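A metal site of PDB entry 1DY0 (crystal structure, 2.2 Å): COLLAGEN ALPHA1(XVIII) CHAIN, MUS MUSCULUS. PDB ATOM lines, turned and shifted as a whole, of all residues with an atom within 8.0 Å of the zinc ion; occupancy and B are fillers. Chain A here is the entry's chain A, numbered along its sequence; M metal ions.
The zinc ion is bound by OD1 of Asp 80 (1.8 Å), NE2 of His 7 (1.9 Å), OD2 of Asp 9 (2.0 Å) and NE2 of His 15 (2.1 Å).
The backbone NH (N) of Asp 80 sits at hydrogen-bond distance from the side-chain amide oxygen (OD1) of Asn 77, at 3.3 Å.
A ring nitrogen (ND1) of His 15 sits at hydrogen-bond distance from the side-chain carboxylate (OE1) of Glu 179, at 2.9 Å.
The nearest printed residue that does not touch the zinc ion is Val 13 (4.5 Å).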
ATOM      1  N   HIS A   7     -16.534  -6.791   0.063  1.00  0.00           N
ATOM      2  CA  HIS A   7     -17.321  -5.770   0.744  1.00  0.00           C
ATOM      3  C   HIS A   7     -18.755  -5.965   0.235  1.00  0.00           C
ATOM      4  O   HIS A   7     -18.969  -6.110  -0.967  1.00  0.00           O
ATOM      5  CB  HIS A   7     -16.809  -4.356   0.380  1.00  0.00           C
ATOM      6  CG  HIS A   7     -17.661  -3.230   0.928  1.00  0.00           C
ATOM      7  ND1 HIS A   7     -17.436  -2.657   2.162  1.00  0.00           N
ATOM      8  CD2 HIS A   7     -18.757  -2.626   0.420  1.00  0.00           C
ATOM      9  CE1 HIS A   7     -18.371  -1.749   2.391  1.00  0.00           C
ATOM     10  NE2 HIS A   7     -19.189  -1.724   1.355  1.00  0.00           N
ATOM     11  N   GLN A   8     -19.705  -6.030   1.153  1.00  0.00           N
ATOM     12  CA  GLN A   8     -21.105  -6.225   0.781  1.00  0.00           C
ATOM     13  C   GLN A   8     -22.016  -5.176   1.404  1.00  0.00           C
ATOM     14  O   GLN A   8     -21.875  -4.856   2.584  1.00  0.00           O
ATOM     15  CB  GLN A   8     -21.597  -7.578   1.287  1.00  0.00           C
ATOM     16  CG  GLN A   8     -21.083  -8.800   0.577  1.00  0.00           C
ATOM     17  CD  GLN A   8     -21.800 -10.046   1.074  1.00  0.00           C
ATOM     18  OE1 GLN A   8     -22.909 -10.350   0.625  1.00  0.00           O
ATOM     19  NE2 GLN A   8     -21.209 -10.710   2.047  1.00  0.00           N
ATOM     20  N   ASP A   9     -23.000  -4.724   0.639  1.00  0.00           N
ATOM     21  CA  ASP A   9     -23.964  -3.722   1.118  1.00  0.00           C
ATOM     22  C   ASP A   9     -25.356  -4.314   0.940  1.00  0.00           C
ATOM     23  O   ASP A   9     -25.662  -4.877  -0.115  1.00  0.00           O
ATOM     24  CB  ASP A   9     -23.854  -2.415   0.322  1.00  0.00           C
ATOM     25  CG  ASP A   9     -22.482  -1.784   0.379  1.00  0.00           C
ATOM     26  OD1 ASP A   9     -21.611  -2.157  -0.428  1.00  0.00           O
ATOM     27  OD2 ASP A   9     -22.270  -0.894   1.225  1.00  0.00           O
ATOM     28  N   PHE A  10     -26.216  -4.150   1.929  1.00  0.00           N
ATOM     29  CA  PHE A  10     -27.556  -4.710   1.835  1.00  0.00           C
ATOM     30  C   PHE A  10     -28.638  -3.631   1.655  1.00  0.00           C
ATOM     31  O   PHE A  10     -29.825  -3.869   1.880  1.00  0.00           O
ATOM     32  CB  PHE A  10     -27.812  -5.650   3.026  1.00  0.00           C
ATOM     33  CG  PHE A  10     -26.805  -6.799   3.110  1.00  0.00           C
ATOM     34  CD1 PHE A  10     -27.040  -7.993   2.444  1.00  0.00           C
ATOM     35  CD2 PHE A  10     -25.615  -6.662   3.832  1.00  0.00           C
ATOM     36  CE1 PHE A  10     -26.100  -9.038   2.472  1.00  0.00           C
ATOM     37  CE2 PHE A  10     -24.668  -7.687   3.868  1.00  0.00           C
ATOM     38  CZ  PHE A  10     -24.912  -8.892   3.189  1.00  0.00           C
ATOM     39  N   GLN A  11     -28.201  -2.461   1.192  1.00  0.00           N
ATOM     40  CA  GLN A  11     -29.049  -1.308   0.939  1.00  0.00           C
ATOM     41  C   GLN A  11     -28.395  -0.564  -0.226  1.00  0.00           C
ATOM     42  O   GLN A  11     -27.172  -0.630  -0.368  1.00  0.00           O
ATOM     43  CB  GLN A  11     -29.080  -0.392   2.164  1.00  0.00           C
ATOM     44  CG  GLN A  11     -30.468   0.100   2.576  1.00  0.00           C
ATOM     45  CD  GLN A  11     -30.933  -0.491   3.897  1.00  0.00           C
ATOM     46  OE1 GLN A  11     -30.138  -1.033   4.675  1.00  0.00           O
ATOM     47  NE2 GLN A  11     -32.233  -0.369   4.176  1.00  0.00           N
ATOM     48  N   VAL A  13     -26.473   2.092  -2.155  1.00  0.00           N
ATOM     49  CA  VAL A  13     -25.541   3.175  -1.809  1.00  0.00           C
ATOM     50  C   VAL A  13     -24.476   3.281  -2.897  1.00  0.00           C
ATOM     51  O   VAL A  13     -24.203   2.297  -3.612  1.00  0.00           O
ATOM     52  CB  VAL A  13     -24.770   2.966  -0.456  1.00  0.00           C
ATOM     53  CG1 VAL A  13     -25.718   2.859   0.715  1.00  0.00           C
ATOM     54  CG2 VAL A  13     -23.879   1.752  -0.518  1.00  0.00           C
ATOM     55  N   LEU A  14     -23.884   4.459  -3.017  1.00  0.00           N
ATOM     56  CA  LEU A  14     -22.826   4.726  -3.970  1.00  0.00           C
ATOM     57  C   LEU A  14     -21.605   5.121  -3.146  1.00  0.00           C
ATOM     58  O   LEU A  14     -21.690   5.991  -2.287  1.00  0.00           O
ATOM     59  CB  LEU A  14     -23.216   5.877  -4.914  1.00  0.00           C
ATOM     60  CG  LEU A  14     -24.378   5.654  -5.892  1.00  0.00           C
ATOM     61  CD1 LEU A  14     -24.600   6.899  -6.705  1.00  0.00           C
ATOM     62  CD2 LEU A  14     -24.081   4.485  -6.807  1.00  0.00           C
ATOM     63  N   HIS A  15     -20.473   4.466  -3.367  1.00  0.00           N
ATOM     64  CA  HIS A  15     -19.264   4.768  -2.605  1.00  0.00           C
ATOM     65  C   HIS A  15     -18.397   5.836  -3.229  1.00  0.00           C
ATOM     66  O   HIS A  15     -18.161   5.836  -4.445  1.00  0.00           O
ATOM     67  CB  HIS A  15     -18.411   3.510  -2.384  1.00  0.00           C
ATOM     68  CG  HIS A  15     -19.085   2.458  -1.551  1.00  0.00           C
ATOM     69  ND1 HIS A  15     -19.976   1.547  -2.081  1.00  0.00           N
ATOM     70  CD2 HIS A  15     -19.001   2.173  -0.226  1.00  0.00           C
ATOM     71  CE1 HIS A  15     -20.417   0.751  -1.120  1.00  0.00           C
ATOM     72  NE2 HIS A  15     -19.847   1.114   0.010  1.00  0.00           N
ATOM     73  N   LEU A  46     -14.203  -4.410  -3.629  1.00  0.00           N
ATOM     74  CA  LEU A  46     -15.396  -3.700  -4.028  1.00  0.00           C
ATOM     75  C   LEU A  46     -15.740  -4.243  -5.412  1.00  0.00           C
ATOM     76  O   LEU A  46     -14.881  -4.338  -6.295  1.00  0.00           O
ATOM     77  CB  LEU A  46     -15.190  -2.183  -4.037  1.00  0.00           C
ATOM     78  CG  LEU A  46     -15.021  -1.507  -2.660  1.00  0.00           C
ATOM     79  CD1 LEU A  46     -14.557  -0.077  -2.830  1.00  0.00           C
ATOM     80  CD2 LEU A  46     -16.328  -1.549  -1.901  1.00  0.00           C
ATOM     81  N   PHE A  50     -15.957   1.569 -10.542  1.00  0.00           N
ATOM     82  CA  PHE A  50     -15.436   2.841 -10.061  1.00  0.00           C
ATOM     83  C   PHE A  50     -14.753   3.698 -11.119  1.00  0.00           C
ATOM     84  O   PHE A  50     -13.952   3.199 -11.922  1.00  0.00           O
ATOM     85  CB  PHE A  50     -14.499   2.633  -8.865  1.00  0.00           C
ATOM     86  CG  PHE A  50     -15.230   2.262  -7.606  1.00  0.00           C
ATOM     87  CD1 PHE A  50     -15.695   0.973  -7.407  1.00  0.00           C
ATOM     88  CD2 PHE A  50     -15.506   3.218  -6.632  1.00  0.00           C
ATOM     89  CE1 PHE A  50     -16.415   0.642  -6.277  1.00  0.00           C
ATOM     90  CE2 PHE A  50     -16.228   2.896  -5.507  1.00  0.00           C
ATOM     91  CZ  PHE A  50     -16.682   1.607  -5.330  1.00  0.00           C
ATOM     92  N   VAL A  76     -21.887   7.233   0.289  1.00  0.00           N
ATOM     93  CA  VAL A  76     -21.248   6.821   1.534  1.00  0.00           C
ATOM     94  C   VAL A  76     -19.747   6.664   1.308  1.00  0.00           C
ATOM     95  O   VAL A  76     -19.286   6.593   0.174  1.00  0.00           O
ATOM     96  CB  VAL A  76     -21.838   5.485   2.048  1.00  0.00           C
ATOM     97  CG1 VAL A  76     -23.351   5.604   2.240  1.00  0.00           C
ATOM     98  CG2 VAL A  76     -21.517   4.353   1.086  1.00  0.00           C
ATOM     99  N   ASN A  77     -18.980   6.657   2.393  1.00  0.00           N
ATOM    100  CA  ASN A  77     -17.540   6.477   2.287  1.00  0.00           C
ATOM    101  C   ASN A  77     -17.204   5.010   2.341  1.00  0.00           C
ATOM    102  O   ASN A  77     -18.095   4.160   2.317  1.00  0.00           O
ATOM    103  CB  ASN A  77     -16.786   7.282   3.364  1.00  0.00           C
ATOM    104  CG  ASN A  77     -17.166   6.903   4.788  1.00  0.00           C
ATOM    105  OD1 ASN A  77     -17.393   5.734   5.094  1.00  0.00           O
ATOM    106  ND2 ASN A  77     -17.195   7.884   5.663  1.00  0.00           N
ATOM    107  N   LEU A  78     -15.925   4.690   2.386  1.00  0.00           N
ATOM    108  CA  LEU A  78     -15.493   3.302   2.428  1.00  0.00           C
ATOM    109  C   LEU A  78     -16.187   2.521   3.533  1.00  0.00           C
ATOM    110  O   LEU A  78     -16.560   1.358   3.346  1.00  0.00           O
ATOM    111  CB  LEU A  78     -13.988   3.221   2.635  1.00  0.00           C
ATOM    112  CG  LEU A  78     -13.451   1.807   2.465  1.00  0.00           C
ATOM    113  CD1 LEU A  78     -13.588   1.394   1.010  1.00  0.00           C
ATOM    114  CD2 LEU A  78     -12.016   1.731   2.951  1.00  0.00           C
ATOM    115  N   LYS A  79     -16.364   3.175   4.679  1.00  0.00           N
ATOM    116  CA  LYS A  79     -16.971   2.553   5.842  1.00  0.00           C
ATOM    117  C   LYS A  79     -18.486   2.699   5.925  1.00  0.00           C
ATOM    118  O   LYS A  79     -19.064   2.543   7.003  1.00  0.00           O
ATOM    119  CB  LYS A  79     -16.292   3.070   7.108  1.00  0.00           C
ATOM    120  CG  LYS A  79     -14.804   2.747   7.175  1.00  0.00           C
ATOM    121  CD  LYS A  79     -14.182   3.221   8.472  1.00  0.00           C
ATOM    122  N   ASP A  80     -19.106   2.974   4.781  1.00  0.00           N
ATOM    123  CA  ASP A  80     -20.549   3.130   4.645  1.00  0.00           C
ATOM    124  C   ASP A  80     -21.196   4.234   5.470  1.00  0.00           C
ATOM    125  O   ASP A  80     -22.400   4.206   5.723  1.00  0.00           O
ATOM    126  CB  ASP A  80     -21.270   1.793   4.853  1.00  0.00           C
ATOM    127  CG  ASP A  80     -20.746   0.714   3.930  1.00  0.00           C
ATOM    128  OD1 ASP A  80     -20.670   0.952   2.712  1.00  0.00           O
ATOM    129  OD2 ASP A  80     -20.382  -0.377   4.416  1.00  0.00           O
ATOM    130  N   GLU A  81     -20.416   5.239   5.851  1.00  0.00           N
ATOM    131  CA  GLU A  81     -20.942   6.373   6.598  1.00  0.00           C
ATOM    132  C   GLU A  81     -21.449   7.362   5.546  1.00  0.00           C
ATOM    133  O   GLU A  81     -20.744   7.650   4.580  1.00  0.00           O
ATOM    134  CB  GLU A  81     -19.842   7.009   7.465  1.00  0.00           C
ATOM    135  CG  GLU A  81     -19.159   6.028   8.421  1.00  0.00           C
ATOM    136  CD  GLU A  81     -17.968   6.634   9.149  1.00  0.00           C
ATOM    137  OE1 GLU A  81     -17.577   7.767   8.835  1.00  0.00           O
ATOM    138  OE2 GLU A  81     -17.407   5.963  10.031  1.00  0.00           O
ATOM    139  N   GLU A 179     -18.625   5.358  -7.532  1.00  0.00           N
ATOM    140  CA  GLU A 179     -19.229   4.170  -8.114  1.00  0.00           C
ATOM    141  C   GLU A 179     -20.276   4.725  -9.070  1.00  0.00           C
ATOM    142  O   GLU A 179     -20.913   5.724  -8.766  1.00  0.00           O
ATOM    143  CB  GLU A 179     -19.881   3.373  -6.995  1.00  0.00           C
ATOM    144  CG  GLU A 179     -20.172   1.932  -7.285  1.00  0.00           C
ATOM    145  CD  GLU A 179     -20.404   1.131  -6.022  1.00  0.00           C
ATOM    146  OE1 GLU A 179     -20.435   1.727  -4.913  1.00  0.00           O
ATOM    147  OE2 GLU A 179     -20.551  -0.102  -6.128  1.00  0.00           O
HETATM  148 ZN    ZN M   1     -20.408  -0.304   1.453  1.00  0.00          ZN
